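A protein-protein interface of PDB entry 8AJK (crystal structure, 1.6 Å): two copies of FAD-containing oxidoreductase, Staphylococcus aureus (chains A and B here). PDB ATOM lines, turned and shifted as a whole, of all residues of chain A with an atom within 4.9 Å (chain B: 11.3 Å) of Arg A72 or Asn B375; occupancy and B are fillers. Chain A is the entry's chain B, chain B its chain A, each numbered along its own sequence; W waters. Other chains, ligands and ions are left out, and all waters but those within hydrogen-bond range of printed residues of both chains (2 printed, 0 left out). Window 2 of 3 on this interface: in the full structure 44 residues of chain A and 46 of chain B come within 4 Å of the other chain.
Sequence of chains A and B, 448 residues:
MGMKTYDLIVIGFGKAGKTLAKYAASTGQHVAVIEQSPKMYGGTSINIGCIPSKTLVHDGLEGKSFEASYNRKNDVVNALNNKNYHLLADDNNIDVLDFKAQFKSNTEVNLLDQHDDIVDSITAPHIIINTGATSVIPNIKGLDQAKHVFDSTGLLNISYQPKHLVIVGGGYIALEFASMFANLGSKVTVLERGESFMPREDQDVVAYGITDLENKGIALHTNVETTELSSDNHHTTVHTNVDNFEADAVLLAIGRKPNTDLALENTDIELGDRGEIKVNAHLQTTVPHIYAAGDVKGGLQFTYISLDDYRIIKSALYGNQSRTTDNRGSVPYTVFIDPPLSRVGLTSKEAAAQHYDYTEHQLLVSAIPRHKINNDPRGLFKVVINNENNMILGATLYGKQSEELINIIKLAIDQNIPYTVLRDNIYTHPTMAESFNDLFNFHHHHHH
O of Ile B373 lies within hydrogen-bond range of ND1 of His A58, 3.0 Å away.
O of Asn B374 lies close to NE2 of His A58.
O of Ile B373 lies within hydrogen-bond range of NH2 of Arg A72, 3.0 Å away.
The guanidinium group (NH1) of Arg A72 is in hydrogen-bond range of the side-chain amide oxygen (OD1) of Asn B375 (3.5 Å).
The guanidinium group (NH1) of Arg A72 is in hydrogen-bond range of the backbone carbonyl oxygen (O) of Lys B372, at 2.9 Å.
ND2 of Asn B374 is in hydrogen-bond range of SD of Met B432, at 3.5 Å.
A ring nitrogen (ND1) of His A58 lies within hydrogen-bond range of the side-chain carboxylate (OD1) of Asp A59 (2.8 Å).
OD1 of Asn B374 is in hydrogen-bond range of NE of Arg B370 (2.9 Å).
The side-chain carboxylate (OD2) of Asp A59 is in salt-bridge range of the guanidinium group (NE) of Arg A72 (2.8 Å).
Among the printed residues, pairs that only touch across the chains: Thr A55 with Ile B373 and Val A76 with Lys B372.
Of chain B, only Lys B372 (2.9 Å), Ile B373 (3.0 Å) and Asn B375 (3.5 Å) come within 4 Å of Arg A72.
Of the printed residues of chain A, Asn B375 touches Arg A72 (3.5 Å).
Of chain B, only Ile B373 (3.0 Å) and Asn B374 (3.5 Å) come within 4 Å of His A58.
No residue of chain B comes within 4 Å of Ala A68.
No residue of chain B comes within 4 Å of Ser A69.
No residue of chain B comes within 4 Å of Asn A71.
Lys A73 touches none of the printed residues of chain B.
No residue of chain B comes within 4 Å of Asn A74.
Printed residues of chain A within 4 Å of Ile B373: Thr A55 (3.5 Å), His A58 (3.0 Å) and Arg A72 (3.0 Å).
Printed residues of chain A within 4 Å of Lys B372: Arg A72 (2.9 Å) and Val A76 (3.7 Å).
Of the printed residues of chain A, Asn B374 touches His A58.
Gly B399 touches none of the printed residues of chain A.
Asp B338 touches none of the printed residues of chain A.
The nearest printed residue of chain A that does not touch Asn B374 is Arg A72 (4.7 Å).
Of the 12 printed residues of chain A, 4 touch a printed residue of chain B.
Printed residues of chain A that touch a printed residue of chain B: Thr A55, His A58, Arg A72 and Val A76.
Hydrophobic or aromatic side chains of chain A that line the printed part of chain B: His A58 and Val A76.
Of the 24 printed residues of chain B, 4 touch a printed residue of chain A.
Printed residues of chain B that touch a printed residue of chain A: Lys B372, Ile B373, Asn B374 and Asn B375.
Hydrophobic or aromatic side chains of chain B that line the printed part of chain A: Ile B373.
Among the printed residues, 7 pairs touch across the chains.
No position is printed for both chains.
Of the 7 pairs that touch across the chains among the printed residues, none has its exchanged pair printed and touching as well.
Water W2 bridges the side-chain carboxylate (OD1) of Asp A59 (2.9 Å) and the side-chain amide nitrogen (ND2) of Asn B375 (3.1 Å).
Water W1 bridges OD1 of Asn B375 and NH1 of Arg A72.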
ATOM      1  N   THR A  55      27.345  -3.048   3.292  1.00  0.00           N
ATOM      2  CA  THR A  55      26.434  -1.910   3.273  1.00  0.00           C
ATOM      3  C   THR A  55      26.054  -1.522   4.696  1.00  0.00           C
ATOM      4  O   THR A  55      26.130  -0.346   5.079  1.00  0.00           O
ATOM      5  CB  THR A  55      25.190  -2.255   2.450  1.00  0.00           C
ATOM      6  OG1 THR A  55      25.574  -2.494   1.097  1.00  0.00           O
ATOM      7  CG2 THR A  55      24.157  -1.104   2.493  1.00  0.00           C
ATOM      8  N   HIS A  58      29.145  -0.065   6.498  1.00  0.00           N
ATOM      9  CA  HIS A  58      29.388   1.300   6.044  1.00  0.00           C
ATOM     10  C   HIS A  58      28.408   2.282   6.677  1.00  0.00           C
ATOM     11  O   HIS A  58      28.810   3.313   7.237  1.00  0.00           O
ATOM     12  CB  HIS A  58      29.286   1.351   4.522  1.00  0.00           C
ATOM     13  CG  HIS A  58      29.361   2.741   3.952  1.00  0.00           C
ATOM     14  ND1 HIS A  58      28.255   3.555   3.822  1.00  0.00           N
ATOM     15  CD2 HIS A  58      30.409   3.449   3.464  1.00  0.00           C
ATOM     16  CE1 HIS A  58      28.623   4.710   3.286  1.00  0.00           C
ATOM     17  NE2 HIS A  58      29.922   4.666   3.050  1.00  0.00           N
ATOM     18  N   ASP A  59      27.114   1.999   6.569  1.00  0.00           N
ATOM     19  CA  ASP A  59      26.112   2.944   7.055  1.00  0.00           C
ATOM     20  C   ASP A  59      26.122   3.060   8.575  1.00  0.00           C
ATOM     21  O   ASP A  59      25.827   4.135   9.108  1.00  0.00           O
ATOM     22  CB  ASP A  59      24.722   2.558   6.558  1.00  0.00           C
ATOM     23  CG  ASP A  59      24.513   2.922   5.100  1.00  0.00           C
ATOM     24  OD1 ASP A  59      25.513   3.272   4.432  1.00  0.00           O
ATOM     25  OD2 ASP A  59      23.350   2.887   4.632  1.00  0.00           O
ATOM     26  N   ALA A  68      17.088   2.803   8.841  1.00  0.00           N
ATOM     27  CA  ALA A  68      17.534   3.415   7.597  1.00  0.00           C
ATOM     28  C   ALA A  68      18.581   2.552   6.904  1.00  0.00           C
ATOM     29  O   ALA A  68      18.617   2.476   5.669  1.00  0.00           O
ATOM     30  CB  ALA A  68      18.086   4.817   7.863  1.00  0.00           C
ATOM     31  N   SER A  69      19.443   1.898   7.683  1.00  0.00           N
ATOM     32  CA  SER A  69      20.501   1.078   7.104  1.00  0.00           C
ATOM     33  C   SER A  69      19.924  -0.179   6.465  1.00  0.00           C
ATOM     34  O   SER A  69      20.288  -0.537   5.333  1.00  0.00           O
ATOM     35  CB  SER A  69      21.529   0.719   8.181  1.00  0.00           C
ATOM     36  OG  SER A  69      22.162   1.887   8.703  1.00  0.00           O
ATOM     37  N   TYR A  70      19.019  -0.866   7.178  1.00  0.00           N
ATOM     38  CA  TYR A  70      18.395  -2.056   6.605  1.00  0.00           C
ATOM     39  C   TYR A  70      17.555  -1.721   5.381  1.00  0.00           C
ATOM     40  O   TYR A  70      17.528  -2.504   4.425  1.00  0.00           O
ATOM     41  CB  TYR A  70      17.553  -2.774   7.665  1.00  0.00           C
ATOM     42  CG  TYR A  70      18.334  -3.896   8.296  1.00  0.00           C
ATOM     43  CD1 TYR A  70      19.381  -3.622   9.172  1.00  0.00           C
ATOM     44  CD2 TYR A  70      18.068  -5.219   7.975  1.00  0.00           C
ATOM     45  CE1 TYR A  70      20.123  -4.645   9.727  1.00  0.00           C
ATOM     46  CE2 TYR A  70      18.794  -6.246   8.536  1.00  0.00           C
ATOM     47  CZ  TYR A  70      19.818  -5.959   9.408  1.00  0.00           C
ATOM     48  OH  TYR A  70      20.542  -6.988   9.956  1.00  0.00           O
ATOM     49  N   ASN A  71      16.889  -0.558   5.374  1.00  0.00           N
ATOM     50  CA  ASN A  71      16.104  -0.160   4.206  1.00  0.00           C
ATOM     51  C   ASN A  71      16.994   0.089   2.995  1.00  0.00           C
ATOM     52  O   ASN A  71      16.666  -0.334   1.878  1.00  0.00           O
ATOM     53  CB  ASN A  71      15.288   1.093   4.516  1.00  0.00           C
ATOM     54  CG  ASN A  71      14.009   0.787   5.262  1.00  0.00           C
ATOM     55  OD1 ASN A  71      13.545  -0.351   5.279  1.00  0.00           O
ATOM     56  ND2 ASN A  71      13.439   1.803   5.899  1.00  0.00           N
ATOM     57  N   ARG A  72      18.117   0.787   3.188  1.00  0.00           N
ATOM     58  CA  ARG A  72      19.011   1.023   2.061  1.00  0.00           C
ATOM     59  C   ARG A  72      19.703  -0.261   1.610  1.00  0.00           C
ATOM     60  O   ARG A  72      19.974  -0.430   0.413  1.00  0.00           O
ATOM     61  CB  ARG A  72      20.042   2.100   2.411  1.00  0.00           C
ATOM     62  CG  ARG A  72      20.646   2.721   1.184  1.00  0.00           C
ATOM     63  CD  ARG A  72      21.682   3.820   1.537  1.00  0.00           C
ATOM     64  NE  ARG A  72      22.972   3.249   1.910  1.00  0.00           N
ATOM     65  CZ  ARG A  72      23.895   2.836   1.046  1.00  0.00           C
ATOM     66  NH1 ARG A  72      23.695   2.881  -0.265  1.00  0.00           N
ATOM     67  NH2 ARG A  72      25.060   2.388   1.509  1.00  0.00           N
ATOM     68  N   LYS A  73      19.994  -1.171   2.546  1.00  0.00           N
ATOM     69  CA  LYS A  73      20.537  -2.472   2.170  1.00  0.00           C
ATOM     70  C   LYS A  73      19.584  -3.204   1.229  1.00  0.00           C
ATOM     71  O   LYS A  73      20.016  -3.794   0.232  1.00  0.00           O
ATOM     72  CB  LYS A  73      20.819  -3.304   3.431  1.00  0.00           C
ATOM     73  CG  LYS A  73      21.296  -4.753   3.174  1.00  0.00           C
ATOM     74  CD  LYS A  73      20.144  -5.736   3.164  1.00  0.00           C
ATOM     75  CE  LYS A  73      19.391  -5.733   4.498  1.00  0.00           C
ATOM     76  NZ  LYS A  73      18.156  -6.554   4.388  1.00  0.00           N
ATOM     77  N   ASN A  74      18.278  -3.146   1.508  1.00  0.00           N
ATOM     78  CA  ASN A  74      17.325  -3.824   0.631  1.00  0.00           C
ATOM     79  C   ASN A  74      17.319  -3.206  -0.756  1.00  0.00           C
ATOM     80  O   ASN A  74      17.233  -3.922  -1.762  1.00  0.00           O
ATOM     81  CB  ASN A  74      15.928  -3.786   1.229  1.00  0.00           C
ATOM     82  CG  ASN A  74      15.806  -4.671   2.426  1.00  0.00           C
ATOM     83  OD1 ASN A  74      16.497  -5.684   2.527  1.00  0.00           O
ATOM     84  ND2 ASN A  74      14.917  -4.310   3.342  1.00  0.00           N
ATOM     85  N   ASP A  75      17.425  -1.879  -0.835  1.00  0.00           N
ATOM     86  CA  ASP A  75      17.484  -1.228  -2.140  1.00  0.00           C
ATOM     87  C   ASP A  75      18.737  -1.630  -2.900  1.00  0.00           C
ATOM     88  O   ASP A  75      18.691  -1.856  -4.117  1.00  0.00           O
ATOM     89  CB  ASP A  75      17.448   0.291  -1.978  1.00  0.00           C
ATOM     90  CG  ASP A  75      16.146   0.791  -1.416  1.00  0.00           C
ATOM     91  OD1 ASP A  75      15.135   0.054  -1.480  1.00  0.00           O
ATOM     92  OD2 ASP A  75      16.133   1.939  -0.923  1.00  0.00           O
ATOM     93  N   VAL A  76      19.873  -1.693  -2.206  1.00  0.00           N
ATOM     94  CA  VAL A  76      21.128  -2.051  -2.859  1.00  0.00           C
ATOM     95  C   VAL A  76      21.051  -3.471  -3.410  1.00  0.00           C
ATOM     96  O   VAL A  76      21.409  -3.728  -4.569  1.00  0.00           O
ATOM     97  CB  VAL A  76      22.306  -1.896  -1.885  1.00  0.00           C
ATOM     98  CG1 VAL A  76      23.547  -2.551  -2.460  1.00  0.00           C
ATOM     99  CG2 VAL A  76      22.579  -0.426  -1.600  1.00  0.00           C
ATOM    100  N   LEU B  61      32.542  16.239   4.977  1.00  0.00           N
ATOM    101  CA  LEU B  61      31.913  15.088   4.332  1.00  0.00           C
ATOM    102  C   LEU B  61      31.053  14.298   5.308  1.00  0.00           C
ATOM    103  O   LEU B  61      30.097  13.632   4.895  1.00  0.00           O
ATOM    104  CB  LEU B  61      32.974  14.179   3.721  1.00  0.00           C
ATOM    105  CG  LEU B  61      33.740  14.752   2.522  1.00  0.00           C
ATOM    106  CD1 LEU B  61      34.923  13.869   2.155  1.00  0.00           C
ATOM    107  CD2 LEU B  61      32.800  14.854   1.336  1.00  0.00           C
ATOM    108  N   ASP B 212      29.601  17.729 -10.774  1.00  0.00           N
ATOM    109  CA  ASP B 212      29.483  17.377  -9.363  1.00  0.00           C
ATOM    110  C   ASP B 212      29.683  18.598  -8.468  1.00  0.00           C
ATOM    111  O   ASP B 212      29.021  18.732  -7.428  1.00  0.00           O
ATOM    112  CB  ASP B 212      30.486  16.274  -9.020  1.00  0.00           C
ATOM    113  CG  ASP B 212      30.113  14.924  -9.635  1.00  0.00           C
ATOM    114  OD1 ASP B 212      28.915  14.680  -9.923  1.00  0.00           O
ATOM    115  OD2 ASP B 212      31.033  14.102  -9.820  1.00  0.00           O
ATOM    116  N   LYS B 216      26.543  20.631  -6.169  1.00  0.00           N
ATOM    117  CA  LYS B 216      26.640  21.106  -4.796  1.00  0.00           C
ATOM    118  C   LYS B 216      26.137  22.530  -4.619  1.00  0.00           C
ATOM    119  O   LYS B 216      26.141  23.029  -3.489  1.00  0.00           O
ATOM    120  CB  LYS B 216      28.084  21.037  -4.313  1.00  0.00           C
ATOM    121  CG  LYS B 216      28.600  19.648  -4.057  1.00  0.00           C
ATOM    122  CD  LYS B 216      30.079  19.738  -3.720  1.00  0.00           C
ATOM    123  CE  LYS B 216      30.672  18.379  -3.476  1.00  0.00           C
ATOM    124  NZ  LYS B 216      29.932  17.683  -2.383  1.00  0.00           N
ATOM    125  N   ASP B 338      35.413  16.692  -4.220  1.00  0.00           N
ATOM    126  CA  ASP B 338      34.553  15.663  -3.629  1.00  0.00           C
ATOM    127  C   ASP B 338      33.764  14.985  -4.740  1.00  0.00           C
ATOM    128  O   ASP B 338      32.762  15.549  -5.220  1.00  0.00           O
ATOM    129  CB  ASP B 338      33.605  16.296  -2.606  1.00  0.00           C
ATOM    130  CG  ASP B 338      32.554  15.326  -2.080  1.00  0.00           C
ATOM    131  OD1 ASP B 338      32.789  14.100  -2.112  1.00  0.00           O
ATOM    132  OD2 ASP B 338      31.472  15.796  -1.657  1.00  0.00           O
ATOM    133  N   PRO B 339      34.131  13.762  -5.158  1.00  0.00           N
ATOM    134  CA  PRO B 339      35.198  12.879  -4.648  1.00  0.00           C
ATOM    135  C   PRO B 339      36.568  13.318  -5.144  1.00  0.00           C
ATOM    136  O   PRO B 339      36.654  14.173  -6.024  1.00  0.00           O
ATOM    137  CB  PRO B 339      34.799  11.508  -5.214  1.00  0.00           C
ATOM    138  CG  PRO B 339      34.154  11.851  -6.523  1.00  0.00           C
ATOM    139  CD  PRO B 339      33.356  13.103  -6.228  1.00  0.00           C
ATOM    140  N   VAL B 365      32.264   5.222 -12.006  1.00  0.00           N
ATOM    141  CA  VAL B 365      32.151   4.733 -10.636  1.00  0.00           C
ATOM    142  C   VAL B 365      30.783   4.095 -10.416  1.00  0.00           C
ATOM    143  O   VAL B 365      30.651   3.135  -9.637  1.00  0.00           O
ATOM    144  CB  VAL B 365      32.438   5.877  -9.639  1.00  0.00           C
ATOM    145  CG1 VAL B 365      31.936   5.503  -8.225  1.00  0.00           C
ATOM    146  CG2 VAL B 365      33.943   6.206  -9.634  1.00  0.00           C
ATOM    147  N   SER B 366      29.758   4.557 -11.148  1.00  0.00           N
ATOM    148  CA  SER B 366      28.433   3.939 -11.042  1.00  0.00           C
ATOM    149  C   SER B 366      28.408   2.510 -11.560  1.00  0.00           C
ATOM    150  O   SER B 366      27.456   1.776 -11.272  1.00  0.00           O
ATOM    151  CB  SER B 366      27.387   4.761 -11.800  1.00  0.00           C
ATOM    152  OG  SER B 366      27.728   4.878 -13.172  1.00  0.00           O
ATOM    153  N   ILE B 368      30.850   0.450 -10.665  1.00  0.00           N
ATOM    154  CA  ILE B 368      31.670  -0.242  -9.674  1.00  0.00           C
ATOM    155  C   ILE B 368      30.757  -0.646  -8.519  1.00  0.00           C
ATOM    156  O   ILE B 368      30.198   0.241  -7.854  1.00  0.00           O
ATOM    157  CB  ILE B 368      32.819   0.659  -9.188  1.00  0.00           C
ATOM    158  CG1 ILE B 368      33.778   0.989 -10.342  1.00  0.00           C
ATOM    159  CG2 ILE B 368      33.578   0.013  -8.025  1.00  0.00           C
ATOM    160  CD1 ILE B 368      34.919   1.968  -9.938  1.00  0.00           C
ATOM    161  N   PRO B 369      30.550  -1.946  -8.262  1.00  0.00           N
ATOM    162  CA  PRO B 369      29.550  -2.325  -7.248  1.00  0.00           C
ATOM    163  C   PRO B 369      29.822  -1.754  -5.870  1.00  0.00           C
ATOM    164  O   PRO B 369      28.868  -1.451  -5.142  1.00  0.00           O
ATOM    165  CB  PRO B 369      29.602  -3.861  -7.250  1.00  0.00           C
ATOM    166  CG  PRO B 369      30.058  -4.213  -8.624  1.00  0.00           C
ATOM    167  CD  PRO B 369      31.047  -3.123  -9.004  1.00  0.00           C
ATOM    168  N   ARG B 370      31.090  -1.577  -5.492  1.00  0.00           N
ATOM    169  CA  ARG B 370      31.402  -0.950  -4.212  1.00  0.00           C
ATOM    170  C   ARG B 370      30.801   0.452  -4.074  1.00  0.00           C
ATOM    171  O   ARG B 370      30.586   0.904  -2.944  1.00  0.00           O
ATOM    172  CB  ARG B 370      32.932  -0.911  -4.013  1.00  0.00           C
ATOM    173  CG  ARG B 370      33.432  -0.074  -2.828  1.00  0.00           C
ATOM    174  CD  ARG B 370      33.233  -0.801  -1.463  1.00  0.00           C
ATOM    175  NE  ARG B 370      33.092   0.176  -0.380  1.00  0.00           N
ATOM    176  CZ  ARG B 370      33.386  -0.060   0.893  1.00  0.00           C
ATOM    177  NH1 ARG B 370      33.844  -1.239   1.287  1.00  0.00           N
ATOM    178  NH2 ARG B 370      33.240   0.920   1.789  1.00  0.00           N
ATOM    179  N   HIS B 371      30.492   1.148  -5.181  1.00  0.00           N
ATOM    180  CA  HIS B 371      29.881   2.476  -5.049  1.00  0.00           C
ATOM    181  C   HIS B 371      28.535   2.406  -4.341  1.00  0.00           C
ATOM    182  O   HIS B 371      28.118   3.385  -3.710  1.00  0.00           O
ATOM    183  CB  HIS B 371      29.703   3.153  -6.418  1.00  0.00           C
ATOM    184  CG  HIS B 371      28.363   2.897  -7.049  1.00  0.00           C
ATOM    185  ND1 HIS B 371      28.125   1.825  -7.879  1.00  0.00           N
ATOM    186  CD2 HIS B 371      27.189   3.570  -6.956  1.00  0.00           C
ATOM    187  CE1 HIS B 371      26.863   1.846  -8.274  1.00  0.00           C
ATOM    188  NE2 HIS B 371      26.271   2.891  -7.726  1.00  0.00           N
ATOM    189  N   LYS B 372      27.839   1.261  -4.443  1.00  0.00           N
ATOM    190  CA  LYS B 372      26.565   1.102  -3.748  1.00  0.00           C
ATOM    191  C   LYS B 372      26.771   1.072  -2.241  1.00  0.00           C
ATOM    192  O   LYS B 372      25.984   1.655  -1.481  1.00  0.00           O
ATOM    193  CB  LYS B 372      25.860  -0.182  -4.203  1.00  0.00           C
ATOM    194  CG  LYS B 372      25.310  -0.166  -5.618  1.00  0.00           C
ATOM    195  CD  LYS B 372      24.195   0.848  -5.781  1.00  0.00           C
ATOM    196  CE  LYS B 372      23.297   0.448  -6.948  1.00  0.00           C
ATOM    197  NZ  LYS B 372      22.157   1.379  -7.115  1.00  0.00           N
ATOM    198  N   ILE B 373      27.826   0.391  -1.792  1.00  0.00           N
ATOM    199  CA  ILE B 373      28.158   0.386  -0.370  1.00  0.00           C
ATOM    200  C   ILE B 373      28.507   1.791   0.103  1.00  0.00           C
ATOM    201  O   ILE B 373      28.079   2.213   1.187  1.00  0.00           O
ATOM    202  CB  ILE B 373      29.300  -0.610  -0.098  1.00  0.00           C
ATOM    203  CG1 ILE B 373      28.802  -2.049  -0.303  1.00  0.00           C
ATOM    204  CG2 ILE B 373      29.899  -0.401   1.288  1.00  0.00           C
ATOM    205  CD1 ILE B 373      29.924  -3.025  -0.378  1.00  0.00           C
ATOM    206  N   ASN B 374      29.273   2.542  -0.717  1.00  0.00           N
ATOM    207  CA  ASN B 374      29.668   3.921  -0.415  1.00  0.00           C
ATOM    208  C   ASN B 374      28.503   4.895  -0.421  1.00  0.00           C
ATOM    209  O   ASN B 374      28.653   6.017   0.087  1.00  0.00           O
ATOM    210  CB  ASN B 374      30.697   4.425  -1.441  1.00  0.00           C
ATOM    211  CG  ASN B 374      31.984   3.632  -1.429  1.00  0.00           C
ATOM    212  OD1 ASN B 374      32.276   2.916  -0.465  1.00  0.00           O
ATOM    213  ND2 ASN B 374      32.800   3.807  -2.472  1.00  0.00           N
ATOM    214  N   ASN B 375      27.384   4.531  -1.046  1.00  0.00           N
ATOM    215  CA  ASN B 375      26.265   5.450  -1.275  1.00  0.00           C
ATOM    216  C   ASN B 375      26.715   6.662  -2.087  1.00  0.00           C
ATOM    217  O   ASN B 375      26.348   7.800  -1.792  1.00  0.00           O
ATOM    218  CB  ASN B 375      25.618   5.884   0.037  1.00  0.00           C
ATOM    219  CG  ASN B 375      24.189   6.359  -0.149  1.00  0.00           C
ATOM    220  OD1 ASN B 375      23.614   6.223  -1.232  1.00  0.00           O
ATOM    221  ND2 ASN B 375      23.588   6.886   0.926  1.00  0.00           N
ATOM    222  N   ASP B 376      27.517   6.411  -3.124  1.00  0.00           N
ATOM    223  CA  ASP B 376      28.061   7.507  -3.919  1.00  0.00           C
ATOM    224  C   ASP B 376      28.340   7.009  -5.331  1.00  0.00           C
ATOM    225  O   ASP B 376      29.291   6.248  -5.532  1.00  0.00           O
ATOM    226  CB  ASP B 376      29.340   8.056  -3.293  1.00  0.00           C
ATOM    227  CG  ASP B 376      29.871   9.271  -4.047  1.00  0.00           C
ATOM    228  OD1 ASP B 376      29.159   9.734  -4.960  1.00  0.00           O
ATOM    229  OD2 ASP B 376      30.984   9.745  -3.738  1.00  0.00           O
ATOM    230  N   PRO B 377      27.528   7.383  -6.321  1.00  0.00           N
ATOM    231  CA  PRO B 377      27.752   6.923  -7.700  1.00  0.00           C
ATOM    232  C   PRO B 377      28.647   7.828  -8.530  1.00  0.00           C
ATOM    233  O   PRO B 377      28.852   7.536  -9.715  1.00  0.00           O
ATOM    234  CB  PRO B 377      26.331   6.922  -8.273  1.00  0.00           C
ATOM    235  CG  PRO B 377      25.683   8.101  -7.582  1.00  0.00           C
ATOM    236  CD  PRO B 377      26.300   8.186  -6.198  1.00  0.00           C
ATOM    237  N   ARG B 378      29.160   8.911  -7.952  1.00  0.00           N
ATOM    238  CA  ARG B 378      29.918   9.899  -8.704  1.00  0.00           C
ATOM    239  C   ARG B 378      31.340   9.434  -8.983  1.00  0.00           C
ATOM    240  O   ARG B 378      32.008   8.855  -8.120  1.00  0.00           O
ATOM    241  CB  ARG B 378      29.949  11.222  -7.939  1.00  0.00           C
ATOM    242  CG  ARG B 378      28.548  11.815  -7.684  1.00  0.00           C
ATOM    243  CD  ARG B 378      28.663  12.988  -6.709  1.00  0.00           C
ATOM    244  NE  ARG B 378      29.331  12.512  -5.501  1.00  0.00           N
ATOM    245  CZ  ARG B 378      30.018  13.283  -4.669  1.00  0.00           C
ATOM    246  NH1 ARG B 378      30.054  14.601  -4.815  1.00  0.00           N
ATOM    247  NH2 ARG B 378      30.714  12.714  -3.689  1.00  0.00           N
ATOM    248  N   GLY B 379      31.807   9.718 -10.196  1.00  0.00           N
ATOM    249  CA  GLY B 379      33.199   9.527 -10.522  1.00  0.00           C
ATOM    250  C   GLY B 379      33.452   8.839 -11.848  1.00  0.00           C
ATOM    251  O   GLY B 379      32.531   8.286 -12.460  1.00  0.00           O
ATOM    252  N   GLY B 399      37.080   9.676  -7.899  1.00  0.00           N
ATOM    253  CA  GLY B 399      36.135   8.864  -7.134  1.00  0.00           C
ATOM    254  C   GLY B 399      36.678   8.524  -5.762  1.00  0.00           C
ATOM    255  O   GLY B 399      37.848   8.723  -5.461  1.00  0.00           O
ATOM    256  N   LYS B 400      35.800   7.972  -4.916  1.00  0.00           N
ATOM    257  CA  LYS B 400      36.206   7.678  -3.540  1.00  0.00           C
ATOM    258  C   LYS B 400      37.380   6.705  -3.491  1.00  0.00           C
ATOM    259  O   LYS B 400      37.477   5.770  -4.299  1.00  0.00           O
ATOM    260  CB  LYS B 400      35.029   7.108  -2.733  1.00  0.00           C
ATOM    261  CG  LYS B 400      34.051   8.175  -2.237  1.00  0.00           C
ATOM    262  CD  LYS B 400      33.200   7.606  -1.101  1.00  0.00           C
ATOM    263  CE  LYS B 400      31.918   8.398  -0.867  1.00  0.00           C
ATOM    264  NZ  LYS B 400      32.036   9.868  -0.953  1.00  0.00           N
ATOM    265  N   GLN B 401      38.271   6.936  -2.520  1.00  0.00           N
ATOM    266  CA  GLN B 401      39.486   6.172  -2.240  1.00  0.00           C
ATOM    267  C   GLN B 401      40.588   6.400  -3.264  1.00  0.00           C
ATOM    268  O   GLN B 401      41.620   5.730  -3.196  1.00  0.00           O
ATOM    269  CB  GLN B 401      39.227   4.655  -2.130  1.00  0.00           C
ATOM    270  CG  GLN B 401      38.077   4.304  -1.173  1.00  0.00           C
ATOM    271  CD  GLN B 401      38.416   4.592   0.279  1.00  0.00           C
ATOM    272  OE1 GLN B 401      38.547   5.745   0.680  1.00  0.00           O
ATOM    273  NE2 GLN B 401      38.494   3.534   1.096  1.00  0.00           N
ATOM    274  N   PRO B 430      34.567  -6.406  -0.491  1.00  0.00           N
ATOM    275  CA  PRO B 430      34.231  -5.420  -1.529  1.00  0.00           C
ATOM    276  C   PRO B 430      35.012  -4.121  -1.345  1.00  0.00           C
ATOM    277  O   PRO B 430      34.969  -3.514  -0.278  1.00  0.00           O
ATOM    278  CB  PRO B 430      32.722  -5.234  -1.344  1.00  0.00           C
ATOM    279  CG  PRO B 430      32.491  -5.500   0.125  1.00  0.00           C
ATOM    280  CD  PRO B 430      33.539  -6.476   0.566  1.00  0.00           C
ATOM    281  N   MET B 432      37.211  -0.554  -3.501  1.00  0.00           N
ATOM    282  CA  MET B 432      37.381   0.200  -4.736  1.00  0.00           C
ATOM    283  C   MET B 432      38.517  -0.379  -5.573  1.00  0.00           C
ATOM    284  O   MET B 432      38.473  -0.323  -6.809  1.00  0.00           O
ATOM    285  CB  MET B 432      37.664   1.672  -4.402  1.00  0.00           C
ATOM    286  CG  MET B 432      36.405   2.439  -3.932  1.00  0.00           C
ATOM    287  SD  MET B 432      34.860   2.393  -4.872  1.00  0.00           S
ATOM    288  CE  MET B 432      35.145   3.684  -6.110  1.00  0.00           C
HETATM  289  O   HOH W   1      23.916   3.735  -3.612  1.00  0.00           O
HETATM  290  O   HOH W   2      25.118   5.938   3.461  1.00  0.00           O
